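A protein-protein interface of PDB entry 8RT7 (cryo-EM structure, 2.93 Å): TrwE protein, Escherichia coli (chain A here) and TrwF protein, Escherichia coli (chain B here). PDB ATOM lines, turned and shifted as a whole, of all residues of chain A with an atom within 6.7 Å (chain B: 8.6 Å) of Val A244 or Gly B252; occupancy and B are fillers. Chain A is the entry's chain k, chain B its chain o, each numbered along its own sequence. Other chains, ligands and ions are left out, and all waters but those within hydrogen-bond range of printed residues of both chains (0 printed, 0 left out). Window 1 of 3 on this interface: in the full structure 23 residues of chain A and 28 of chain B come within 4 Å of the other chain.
OH of Tyr A238 is in hydrogen-bond range of ND2 of Asn B249 (3.2 Å). The backbone NH of Ala B254 sits at hydrogen-bond distance from the backbone carbonyl oxygen of Arg A243. The backbone NH (N) of Val A245 lies within hydrogen-bond range of the backbone carbonyl oxygen (O) of Gly B252 (2.8 Å). NH2 of Arg B260 is in salt-bridge range of OD1 of Asp A248. The backbone NH (N) of Val B261 is in hydrogen-bond range of the backbone carbonyl oxygen (O) of Ser A388 (2.8 Å). O of Val A245 sits close to NH2 of Arg B260, 2.2 Å away.
The side-chain hydroxyl (OG) of Ser A239 lies within hydrogen-bond range of the backbone NH (N) of Gly A242, 3.4 Å away. O of Val A244 is in hydrogen-bond range of N of Ser A239, at 2.8 Å. The backbone carbonyl oxygen of Leu A246 is in hydrogen-bond range of the side-chain hydroxyl of Tyr A387 (3.1 Å). The guanidinium group (NH1) of Arg B178 lies close to the side-chain amide nitrogen (ND2) of Asn B249, at 3.4 Å. O of Thr B253 lies within hydrogen-bond range of NH1 of Arg B178, at 3.3 Å. The backbone carbonyl oxygen of Ser B255 sits at hydrogen-bond distance from the side-chain hydroxyl of Thr B253, 2.9 Å away.
Among the printed residues, pairs that only touch across the chains: Tyr A238 with Arg B178 (3.3 Å), Tyr A238 with Phe B179 (3.9 Å), Gly A242 with Phe B179 (3.5 Å), Gly A242 with Ala B254 (3.9 Å), Arg A243 with Phe B148 (3.6 Å), Arg A243 with Thr B253 (3.2 Å), Val A244 with Gly B252 (3.8 Å), Val A244 with Arg B260 (3.9 Å), Val A245 with Asn B249 (3.5 Å), Tyr A387 with Arg B260 (3.5 Å), Tyr A387 with Val B261 (3.4 Å), Ser A388 with Arg B259 (3.8 Å), Ser A388 with Arg B260 (3.5 Å), Leu A389 with Val B144 (3.6 Å), Leu A389 with Thr B253 (3.9 Å) and Leu A389 with Arg B259 (3.4 Å).
Of chain B, only Gly B252 and Arg B260 come within 4 Å of Val A244. Of chain A, only Val A244 (3.8 Å) and Val A245 (2.8 Å) come within 4 Å of Gly B252. Printed residues of chain A within 4 Å of Val B261: Tyr A387 (3.4 Å) and Ser A388 (2.8 Å). Printed residues of chain A within 4 Å of Thr B253: Arg A243 (3.2 Å) and Leu A389 (3.9 Å). Of the printed residues of chain B, Gly A242 touches Phe B179 and Ala B254. Of the printed residues of chain A, Arg B178 touches Tyr A238 (3.3 Å). Of the printed residues of chain A, Phe B148 touches Arg A243. Arg A203 touches none of the printed residues of chain B. The nearest residue of chain B that does not touch Val A244 is Thr B253 (4.1 Å).
Hydrophobic or aromatic side chains of chain B within 4 Å of the printed part of chain A: Val B144, Phe B148, Phe B179, Ala B254 and Val B261. Hydrophobic or aromatic side chains of chain A within 4 Å of the printed part of chain B: Tyr A238, Val A244, Val A245, Tyr A387 and Leu A389.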
ATOM      1  N   ARG A 203     -28.151  18.091  23.939  1.00  0.00           N
ATOM      2  CA  ARG A 203     -27.499  17.481  22.795  1.00  0.00           C
ATOM      3  C   ARG A 203     -26.781  18.489  21.923  1.00  0.00           C
ATOM      4  O   ARG A 203     -26.241  18.106  20.886  1.00  0.00           O
ATOM      5  CB  ARG A 203     -28.518  16.713  21.963  1.00  0.00           C
ATOM      6  CG  ARG A 203     -28.981  15.433  22.610  1.00  0.00           C
ATOM      7  CD  ARG A 203     -30.164  14.876  21.883  1.00  0.00           C
ATOM      8  NE  ARG A 203     -29.826  14.551  20.509  1.00  0.00           N
ATOM      9  CZ  ARG A 203     -30.399  15.107  19.452  1.00  0.00           C
ATOM     10  NH1 ARG A 203     -31.346  16.015  19.610  1.00  0.00           N
ATOM     11  NH2 ARG A 203     -30.026  14.746  18.239  1.00  0.00           N
ATOM     12  N   ASP A 204     -26.771  19.762  22.304  1.00  0.00           N
ATOM     13  CA  ASP A 204     -26.004  20.761  21.577  1.00  0.00           C
ATOM     14  C   ASP A 204     -24.626  20.977  22.162  1.00  0.00           C
ATOM     15  O   ASP A 204     -23.771  21.554  21.490  1.00  0.00           O
ATOM     16  CB  ASP A 204     -26.743  22.096  21.547  1.00  0.00           C
ATOM     17  CG  ASP A 204     -27.758  22.171  20.442  1.00  0.00           C
ATOM     18  OD1 ASP A 204     -27.485  21.648  19.347  1.00  0.00           O
ATOM     19  OD2 ASP A 204     -28.832  22.759  20.659  1.00  0.00           O
ATOM     20  N   MET A 205     -24.398  20.541  23.393  1.00  0.00           N
ATOM     21  CA  MET A 205     -23.086  20.611  24.012  1.00  0.00           C
ATOM     22  C   MET A 205     -22.631  19.216  24.379  1.00  0.00           C
ATOM     23  O   MET A 205     -22.153  18.986  25.488  1.00  0.00           O
ATOM     24  CB  MET A 205     -23.102  21.498  25.253  1.00  0.00           C
ATOM     25  CG  MET A 205     -23.724  22.841  25.051  1.00  0.00           C
ATOM     26  SD  MET A 205     -22.664  23.957  24.141  1.00  0.00           S
ATOM     27  CE  MET A 205     -23.889  25.084  23.518  1.00  0.00           C
ATOM     28  N   VAL A 237     -15.660  19.037  14.524  1.00  0.00           N
ATOM     29  CA  VAL A 237     -16.472  17.990  15.124  1.00  0.00           C
ATOM     30  C   VAL A 237     -17.699  18.661  15.712  1.00  0.00           C
ATOM     31  O   VAL A 237     -17.580  19.543  16.565  1.00  0.00           O
ATOM     32  CB  VAL A 237     -15.695  17.200  16.187  1.00  0.00           C
ATOM     33  CG1 VAL A 237     -16.557  16.144  16.790  1.00  0.00           C
ATOM     34  CG2 VAL A 237     -14.483  16.557  15.579  1.00  0.00           C
ATOM     35  N   TYR A 238     -18.872  18.268  15.245  1.00  0.00           N
ATOM     36  CA  TYR A 238     -20.106  18.896  15.676  1.00  0.00           C
ATOM     37  C   TYR A 238     -20.709  18.137  16.847  1.00  0.00           C
ATOM     38  O   TYR A 238     -20.267  17.050  17.214  1.00  0.00           O
ATOM     39  CB  TYR A 238     -21.101  18.966  14.525  1.00  0.00           C
ATOM     40  CG  TYR A 238     -20.768  20.013  13.510  1.00  0.00           C
ATOM     41  CD1 TYR A 238     -19.749  19.825  12.610  1.00  0.00           C
ATOM     42  CD2 TYR A 238     -21.466  21.196  13.462  1.00  0.00           C
ATOM     43  CE1 TYR A 238     -19.445  20.774  11.689  1.00  0.00           C
ATOM     44  CE2 TYR A 238     -21.167  22.153  12.544  1.00  0.00           C
ATOM     45  CZ  TYR A 238     -20.150  21.940  11.663  1.00  0.00           C
ATOM     46  OH  TYR A 238     -19.840  22.899  10.736  1.00  0.00           O
ATOM     47  N   SER A 239     -21.734  18.731  17.440  1.00  0.00           N
ATOM     48  CA  SER A 239     -22.464  18.083  18.511  1.00  0.00           C
ATOM     49  C   SER A 239     -23.292  16.926  17.960  1.00  0.00           C
ATOM     50  O   SER A 239     -23.372  16.705  16.751  1.00  0.00           O
ATOM     51  CB  SER A 239     -23.347  19.100  19.220  1.00  0.00           C
ATOM     52  OG  SER A 239     -24.175  19.775  18.302  1.00  0.00           O
ATOM     53  N   THR A 240     -23.909  16.162  18.866  1.00  0.00           N
ATOM     54  CA  THR A 240     -24.781  15.080  18.423  1.00  0.00           C
ATOM     55  C   THR A 240     -26.000  15.622  17.702  1.00  0.00           C
ATOM     56  O   THR A 240     -26.488  15.011  16.748  1.00  0.00           O
ATOM     57  CB  THR A 240     -25.204  14.212  19.600  1.00  0.00           C
ATOM     58  OG1 THR A 240     -25.914  15.001  20.552  1.00  0.00           O
ATOM     59  CG2 THR A 240     -24.009  13.645  20.249  1.00  0.00           C
ATOM     60  N   SER A 241     -26.514  16.764  18.145  1.00  0.00           N
ATOM     61  CA  SER A 241     -27.543  17.439  17.374  1.00  0.00           C
ATOM     62  C   SER A 241     -27.024  17.890  16.021  1.00  0.00           C
ATOM     63  O   SER A 241     -27.818  18.086  15.099  1.00  0.00           O
ATOM     64  CB  SER A 241     -28.077  18.633  18.150  1.00  0.00           C
ATOM     65  OG  SER A 241     -27.032  19.516  18.487  1.00  0.00           O
ATOM     66  N   GLY A 242     -25.714  18.044  15.879  1.00  0.00           N
ATOM     67  CA  GLY A 242     -25.129  18.464  14.624  1.00  0.00           C
ATOM     68  C   GLY A 242     -25.333  19.926  14.316  1.00  0.00           C
ATOM     69  O   GLY A 242     -25.452  20.294  13.144  1.00  0.00           O
ATOM     70  N   ARG A 243     -25.375  20.773  15.340  1.00  0.00           N
ATOM     71  CA  ARG A 243     -25.630  22.194  15.158  1.00  0.00           C
ATOM     72  C   ARG A 243     -24.561  23.105  15.727  1.00  0.00           C
ATOM     73  O   ARG A 243     -24.514  24.272  15.333  1.00  0.00           O
ATOM     74  CB  ARG A 243     -26.973  22.584  15.786  1.00  0.00           C
ATOM     75  CG  ARG A 243     -28.124  21.731  15.340  1.00  0.00           C
ATOM     76  CD  ARG A 243     -29.443  22.309  15.767  1.00  0.00           C
ATOM     77  NE  ARG A 243     -29.505  22.515  17.205  1.00  0.00           N
ATOM     78  CZ  ARG A 243     -30.604  22.875  17.854  1.00  0.00           C
ATOM     79  NH1 ARG A 243     -30.578  23.053  19.163  1.00  0.00           N
ATOM     80  NH2 ARG A 243     -31.733  23.055  17.188  1.00  0.00           N
ATOM     81  N   VAL A 244     -23.714  22.634  16.633  1.00  0.00           N
ATOM     82  CA  VAL A 244     -22.676  23.446  17.252  1.00  0.00           C
ATOM     83  C   VAL A 244     -21.346  22.737  17.070  1.00  0.00           C
ATOM     84  O   VAL A 244     -21.257  21.521  17.253  1.00  0.00           O
ATOM     85  CB  VAL A 244     -22.959  23.687  18.747  1.00  0.00           C
ATOM     86  CG1 VAL A 244     -21.978  24.660  19.322  1.00  0.00           C
ATOM     87  CG2 VAL A 244     -24.362  24.181  18.940  1.00  0.00           C
ATOM     88  N   VAL A 245     -20.315  23.491  16.701  1.00  0.00           N
ATOM     89  CA  VAL A 245     -18.971  22.939  16.586  1.00  0.00           C
ATOM     90  C   VAL A 245     -18.372  22.881  17.983  1.00  0.00           C
ATOM     91  O   VAL A 245     -18.111  23.914  18.596  1.00  0.00           O
ATOM     92  CB  VAL A 245     -18.091  23.768  15.650  1.00  0.00           C
ATOM     93  CG1 VAL A 245     -16.785  23.077  15.448  1.00  0.00           C
ATOM     94  CG2 VAL A 245     -18.770  23.981  14.343  1.00  0.00           C
ATOM     95  N   LEU A 246     -18.140  21.678  18.484  1.00  0.00           N
ATOM     96  CA  LEU A 246     -17.633  21.516  19.833  1.00  0.00           C
ATOM     97  C   LEU A 246     -16.137  21.280  19.884  1.00  0.00           C
ATOM     98  O   LEU A 246     -15.502  21.630  20.879  1.00  0.00           O
ATOM     99  CB  LEU A 246     -18.357  20.369  20.527  1.00  0.00           C
ATOM    100  CG  LEU A 246     -19.841  20.626  20.726  1.00  0.00           C
ATOM    101  CD1 LEU A 246     -20.401  19.533  21.549  1.00  0.00           C
ATOM    102  CD2 LEU A 246     -20.081  21.949  21.391  1.00  0.00           C
ATOM    103  N   LEU A 247     -15.558  20.706  18.839  1.00  0.00           N
ATOM    104  CA  LEU A 247     -14.113  20.594  18.705  1.00  0.00           C
ATOM    105  C   LEU A 247     -13.727  21.143  17.346  1.00  0.00           C
ATOM    106  O   LEU A 247     -14.136  20.601  16.319  1.00  0.00           O
ATOM    107  CB  LEU A 247     -13.644  19.150  18.858  1.00  0.00           C
ATOM    108  CG  LEU A 247     -13.879  18.544  20.231  1.00  0.00           C
ATOM    109  CD1 LEU A 247     -13.669  17.063  20.179  1.00  0.00           C
ATOM    110  CD2 LEU A 247     -12.961  19.172  21.236  1.00  0.00           C
ATOM    111  N   ASP A 248     -12.930  22.201  17.343  1.00  0.00           N
ATOM    112  CA  ASP A 248     -12.573  22.915  16.135  1.00  0.00           C
ATOM    113  C   ASP A 248     -11.546  22.135  15.333  1.00  0.00           C
ATOM    114  O   ASP A 248     -10.917  21.200  15.823  1.00  0.00           O
ATOM    115  CB  ASP A 248     -12.011  24.279  16.493  1.00  0.00           C
ATOM    116  CG  ASP A 248     -13.047  25.191  17.065  1.00  0.00           C
ATOM    117  OD1 ASP A 248     -14.229  25.042  16.703  1.00  0.00           O
ATOM    118  OD2 ASP A 248     -12.686  26.044  17.901  1.00  0.00           O
ATOM    119  N   TYR A 387     -19.003  26.522  26.624  1.00  0.00           N
ATOM    120  CA  TYR A 387     -19.614  27.235  25.518  1.00  0.00           C
ATOM    121  C   TYR A 387     -21.021  27.660  25.898  1.00  0.00           C
ATOM    122  O   TYR A 387     -21.649  27.085  26.786  1.00  0.00           O
ATOM    123  CB  TYR A 387     -19.713  26.387  24.249  1.00  0.00           C
ATOM    124  CG  TYR A 387     -18.419  25.889  23.670  1.00  0.00           C
ATOM    125  CD1 TYR A 387     -17.442  26.760  23.254  1.00  0.00           C
ATOM    126  CD2 TYR A 387     -18.196  24.537  23.513  1.00  0.00           C
ATOM    127  CE1 TYR A 387     -16.281  26.298  22.718  1.00  0.00           C
ATOM    128  CE2 TYR A 387     -17.042  24.073  22.983  1.00  0.00           C
ATOM    129  CZ  TYR A 387     -16.088  24.953  22.585  1.00  0.00           C
ATOM    130  OH  TYR A 387     -14.925  24.479  22.048  1.00  0.00           O
ATOM    131  N   SER A 388     -21.511  28.671  25.191  1.00  0.00           N
ATOM    132  CA  SER A 388     -22.917  29.035  25.210  1.00  0.00           C
ATOM    133  C   SER A 388     -23.255  29.604  23.847  1.00  0.00           C
ATOM    134  O   SER A 388     -22.368  29.948  23.070  1.00  0.00           O
ATOM    135  CB  SER A 388     -23.240  30.028  26.326  1.00  0.00           C
ATOM    136  OG  SER A 388     -22.505  31.226  26.183  1.00  0.00           O
ATOM    137  N   LEU A 389     -24.543  29.675  23.547  1.00  0.00           N
ATOM    138  CA  LEU A 389     -25.008  30.115  22.243  1.00  0.00           C
ATOM    139  C   LEU A 389     -25.761  31.427  22.368  1.00  0.00           C
ATOM    140  O   LEU A 389     -26.569  31.606  23.280  1.00  0.00           O
ATOM    141  CB  LEU A 389     -25.916  29.074  21.597  1.00  0.00           C
ATOM    142  CG  LEU A 389     -25.436  27.629  21.583  1.00  0.00           C
ATOM    143  CD1 LEU A 389     -26.569  26.718  21.195  1.00  0.00           C
ATOM    144  CD2 LEU A 389     -24.270  27.464  20.646  1.00  0.00           C
ATOM    145  N   VAL B 144     -32.035  31.797  19.965  1.00  0.00           N
ATOM    146  CA  VAL B 144     -31.158  30.804  19.349  1.00  0.00           C
ATOM    147  C   VAL B 144     -31.964  29.693  18.698  1.00  0.00           C
ATOM    148  O   VAL B 144     -31.646  29.245  17.588  1.00  0.00           O
ATOM    149  CB  VAL B 144     -30.169  30.253  20.392  1.00  0.00           C
ATOM    150  CG1 VAL B 144     -29.358  29.159  19.802  1.00  0.00           C
ATOM    151  CG2 VAL B 144     -29.226  31.346  20.815  1.00  0.00           C
ATOM    152  N   PHE B 148     -31.856  28.815  14.686  1.00  0.00           N
ATOM    153  CA  PHE B 148     -31.600  27.532  14.034  1.00  0.00           C
ATOM    154  C   PHE B 148     -32.740  27.159  13.102  1.00  0.00           C
ATOM    155  O   PHE B 148     -32.512  26.783  11.949  1.00  0.00           O
ATOM    156  CB  PHE B 148     -31.366  26.389  15.023  1.00  0.00           C
ATOM    157  CG  PHE B 148     -30.056  26.440  15.738  1.00  0.00           C
ATOM    158  CD1 PHE B 148     -28.894  26.122  15.066  1.00  0.00           C
ATOM    159  CD2 PHE B 148     -29.997  26.607  17.099  1.00  0.00           C
ATOM    160  CE1 PHE B 148     -27.692  26.118  15.705  1.00  0.00           C
ATOM    161  CE2 PHE B 148     -28.789  26.574  17.749  1.00  0.00           C
ATOM    162  CZ  PHE B 148     -27.639  26.332  17.051  1.00  0.00           C
ATOM    163  N   ARG B 178     -22.316  23.173   3.754  1.00  0.00           N
ATOM    164  CA  ARG B 178     -21.777  22.778   5.044  1.00  0.00           C
ATOM    165  C   ARG B 178     -21.924  21.288   5.287  1.00  0.00           C
ATOM    166  O   ARG B 178     -20.951  20.630   5.669  1.00  0.00           O
ATOM    167  CB  ARG B 178     -22.473  23.580   6.156  1.00  0.00           C
ATOM    168  CG  ARG B 178     -21.902  23.415   7.551  1.00  0.00           C
ATOM    169  CD  ARG B 178     -20.525  24.030   7.684  1.00  0.00           C
ATOM    170  NE  ARG B 178     -20.490  25.421   7.251  1.00  0.00           N
ATOM    171  CZ  ARG B 178     -20.900  26.444   7.989  1.00  0.00           C
ATOM    172  NH1 ARG B 178     -21.387  26.237   9.200  1.00  0.00           N
ATOM    173  NH2 ARG B 178     -20.828  27.673   7.512  1.00  0.00           N
ATOM    174  N   PHE B 179     -23.111  20.732   5.057  1.00  0.00           N
ATOM    175  CA  PHE B 179     -23.380  19.309   5.173  1.00  0.00           C
ATOM    176  C   PHE B 179     -23.835  18.777   3.826  1.00  0.00           C
ATOM    177  O   PHE B 179     -24.273  19.532   2.964  1.00  0.00           O
ATOM    178  CB  PHE B 179     -24.469  19.017   6.209  1.00  0.00           C
ATOM    179  CG  PHE B 179     -24.059  19.256   7.624  1.00  0.00           C
ATOM    180  CD1 PHE B 179     -22.786  19.656   7.942  1.00  0.00           C
ATOM    181  CD2 PHE B 179     -24.958  19.071   8.643  1.00  0.00           C
ATOM    182  CE1 PHE B 179     -22.427  19.871   9.240  1.00  0.00           C
ATOM    183  CE2 PHE B 179     -24.595  19.284   9.943  1.00  0.00           C
ATOM    184  CZ  PHE B 179     -23.333  19.680  10.237  1.00  0.00           C
ATOM    185  N   HIS B 220     -21.317  15.472   7.777  1.00  0.00           N
ATOM    186  CA  HIS B 220     -20.824  16.762   8.229  1.00  0.00           C
ATOM    187  C   HIS B 220     -19.681  17.283   7.378  1.00  0.00           C
ATOM    188  O   HIS B 220     -18.769  17.928   7.902  1.00  0.00           O
ATOM    189  CB  HIS B 220     -20.397  16.668   9.690  1.00  0.00           C
ATOM    190  CG  HIS B 220     -21.509  16.327  10.630  1.00  0.00           C
ATOM    191  ND1 HIS B 220     -22.836  16.456  10.292  1.00  0.00           N
ATOM    192  CD2 HIS B 220     -21.488  15.882  11.905  1.00  0.00           C
ATOM    193  CE1 HIS B 220     -23.585  16.097  11.316  1.00  0.00           C
ATOM    194  NE2 HIS B 220     -22.792  15.742  12.306  1.00  0.00           N
ATOM    195  N   PRO B 248     -17.033  29.898   4.745  1.00  0.00           N
ATOM    196  CA  PRO B 248     -16.321  29.722   6.013  1.00  0.00           C
ATOM    197  C   PRO B 248     -17.244  29.795   7.216  1.00  0.00           C
ATOM    198  O   PRO B 248     -18.251  30.504   7.220  1.00  0.00           O
ATOM    199  CB  PRO B 248     -15.314  30.874   6.016  1.00  0.00           C
ATOM    200  CG  PRO B 248     -15.828  31.842   5.031  1.00  0.00           C
ATOM    201  CD  PRO B 248     -16.530  31.054   3.989  1.00  0.00           C
ATOM    202  N   ASN B 249     -16.866  29.057   8.259  1.00  0.00           N
ATOM    203  CA  ASN B 249     -17.676  28.895   9.462  1.00  0.00           C
ATOM    204  C   ASN B 249     -17.160  29.834  10.546  1.00  0.00           C
ATOM    205  O   ASN B 249     -16.457  29.436  11.471  1.00  0.00           O
ATOM    206  CB  ASN B 249     -17.639  27.447   9.923  1.00  0.00           C
ATOM    207  CG  ASN B 249     -18.655  27.151  10.995  1.00  0.00           C
ATOM    208  OD1 ASN B 249     -19.329  28.044  11.493  1.00  0.00           O
ATOM    209  ND2 ASN B 249     -18.766  25.886  11.363  1.00  0.00           N
ATOM    210  N   ASP B 250     -17.544  31.102  10.441  1.00  0.00           N
ATOM    211  CA  ASP B 250     -17.077  32.100  11.391  1.00  0.00           C
ATOM    212  C   ASP B 250     -17.842  32.083  12.704  1.00  0.00           C
ATOM    213  O   ASP B 250     -17.389  32.704  13.669  1.00  0.00           O
ATOM    214  CB  ASP B 250     -17.177  33.492  10.779  1.00  0.00           C
ATOM    215  CG  ASP B 250     -16.477  33.593   9.451  1.00  0.00           C
ATOM    216  OD1 ASP B 250     -15.231  33.575   9.430  1.00  0.00           O
ATOM    217  OD2 ASP B 250     -17.174  33.698   8.422  1.00  0.00           O
ATOM    218  N   THR B 251     -18.974  31.390  12.776  1.00  0.00           N
ATOM    219  CA  THR B 251     -19.836  31.459  13.945  1.00  0.00           C
ATOM    220  C   THR B 251     -19.653  30.308  14.917  1.00  0.00           C
ATOM    221  O   THR B 251     -20.016  30.450  16.086  1.00  0.00           O
ATOM    222  CB  THR B 251     -21.306  31.509  13.519  1.00  0.00           C
ATOM    223  OG1 THR B 251     -21.564  30.485  12.556  1.00  0.00           O
ATOM    224  CG2 THR B 251     -21.625  32.845  12.911  1.00  0.00           C
ATOM    225  N   GLY B 252     -19.108  29.181  14.479  1.00  0.00           N
ATOM    226  CA  GLY B 252     -18.945  28.044  15.355  1.00  0.00           C
ATOM    227  C   GLY B 252     -20.166  27.170  15.503  1.00  0.00           C
ATOM    228  O   GLY B 252     -20.142  26.239  16.308  1.00  0.00           O
ATOM    229  N   THR B 253     -21.235  27.447  14.766  1.00  0.00           N
ATOM    230  CA  THR B 253     -22.430  26.623  14.747  1.00  0.00           C
ATOM    231  C   THR B 253     -22.726  26.239  13.307  1.00  0.00           C
ATOM    232  O   THR B 253     -21.959  26.542  12.393  1.00  0.00           O
ATOM    233  CB  THR B 253     -23.628  27.349  15.366  1.00  0.00           C
ATOM    234  OG1 THR B 253     -23.825  28.595  14.698  1.00  0.00           O
ATOM    235  CG2 THR B 253     -23.398  27.609  16.830  1.00  0.00           C
ATOM    236  N   ALA B 254     -23.853  25.568  13.099  1.00  0.00           N
ATOM    237  CA  ALA B 254     -24.249  25.166  11.760  1.00  0.00           C
ATOM    238  C   ALA B 254     -24.953  26.271  10.992  1.00  0.00           C
ATOM    239  O   ALA B 254     -25.146  26.131   9.781  1.00  0.00           O
ATOM    240  CB  ALA B 254     -25.156  23.939  11.822  1.00  0.00           C
ATOM    241  N   SER B 255     -25.336  27.358  11.650  1.00  0.00           N
ATOM    242  CA  SER B 255     -26.007  28.429  10.942  1.00  0.00           C
ATOM    243  C   SER B 255     -25.283  29.744  11.172  1.00  0.00           C
ATOM    244  O   SER B 255     -24.661  29.938  12.218  1.00  0.00           O
ATOM    245  CB  SER B 255     -27.464  28.578  11.393  1.00  0.00           C
ATOM    246  OG  SER B 255     -27.534  29.168  12.673  1.00  0.00           O
ATOM    247  N   PRO B 256     -25.347  30.668  10.211  1.00  0.00           N
ATOM    248  CA  PRO B 256     -24.724  31.982  10.405  1.00  0.00           C
ATOM    249  C   PRO B 256     -25.493  32.895  11.338  1.00  0.00           C
ATOM    250  O   PRO B 256     -25.002  33.984  11.646  1.00  0.00           O
ATOM    251  CB  PRO B 256     -24.684  32.561   8.985  1.00  0.00           C
ATOM    252  CG  PRO B 256     -24.997  31.424   8.075  1.00  0.00           C
ATOM    253  CD  PRO B 256     -25.851  30.501   8.844  1.00  0.00           C
ATOM    254  N   VAL B 258     -26.460  32.058  14.481  1.00  0.00           N
ATOM    255  CA  VAL B 258     -26.190  31.707  15.868  1.00  0.00           C
ATOM    256  C   VAL B 258     -24.683  31.704  16.061  1.00  0.00           C
ATOM    257  O   VAL B 258     -23.948  31.240  15.187  1.00  0.00           O
ATOM    258  CB  VAL B 258     -26.787  30.339  16.249  1.00  0.00           C
ATOM    259  CG1 VAL B 258     -26.603  30.072  17.721  1.00  0.00           C
ATOM    260  CG2 VAL B 258     -28.242  30.282  15.897  1.00  0.00           C
ATOM    261  N   ARG B 259     -24.229  32.219  17.195  1.00  0.00           N
ATOM    262  CA  ARG B 259     -22.816  32.339  17.512  1.00  0.00           C
ATOM    263  C   ARG B 259     -22.487  31.505  18.744  1.00  0.00           C
ATOM    264  O   ARG B 259     -23.255  31.483  19.708  1.00  0.00           O
ATOM    265  CB  ARG B 259     -22.456  33.805  17.752  1.00  0.00           C
ATOM    266  CG  ARG B 259     -21.091  34.037  18.339  1.00  0.00           C
ATOM    267  CD  ARG B 259     -20.481  35.308  17.808  1.00  0.00           C
ATOM    268  NE  ARG B 259     -19.879  35.120  16.495  1.00  0.00           N
ATOM    269  CZ  ARG B 259     -19.782  36.077  15.580  1.00  0.00           C
ATOM    270  NH1 ARG B 259     -19.221  35.824  14.409  1.00  0.00           N
ATOM    271  NH2 ARG B 259     -20.256  37.287  15.839  1.00  0.00           N
ATOM    272  N   ARG B 260     -21.354  30.818  18.712  1.00  0.00           N
ATOM    273  CA  ARG B 260     -20.874  30.049  19.852  1.00  0.00           C
ATOM    274  C   ARG B 260     -19.851  30.882  20.608  1.00  0.00           C
ATOM    275  O   ARG B 260     -18.781  31.187  20.073  1.00  0.00           O
ATOM    276  CB  ARG B 260     -20.253  28.733  19.399  1.00  0.00           C
ATOM    277  CG  ARG B 260     -19.874  27.818  20.524  1.00  0.00           C
ATOM    278  CD  ARG B 260     -18.837  26.847  20.069  1.00  0.00           C
ATOM    279  NE  ARG B 260     -17.664  27.530  19.552  1.00  0.00           N
ATOM    280  CZ  ARG B 260     -16.648  26.922  18.961  1.00  0.00           C
ATOM    281  NH1 ARG B 260     -15.622  27.624  18.519  1.00  0.00           N
ATOM    282  NH2 ARG B 260     -16.664  25.614  18.806  1.00  0.00           N
ATOM    283  N   VAL B 261     -20.166  31.237  21.848  1.00  0.00           N
ATOM    284  CA  VAL B 261     -19.335  32.147  22.621  1.00  0.00           C
ATOM    285  C   VAL B 261     -18.710  31.394  23.784  1.00  0.00           C
ATOM    286  O   VAL B 261     -19.257  30.407  24.281  1.00  0.00           O
ATOM    287  CB  VAL B 261     -20.135  33.371  23.111  1.00  0.00           C
ATOM    288  CG1 VAL B 261     -20.439  34.279  21.952  1.00  0.00           C
ATOM    289  CG2 VAL B 261     -21.412  32.945  23.747  1.00  0.00           C
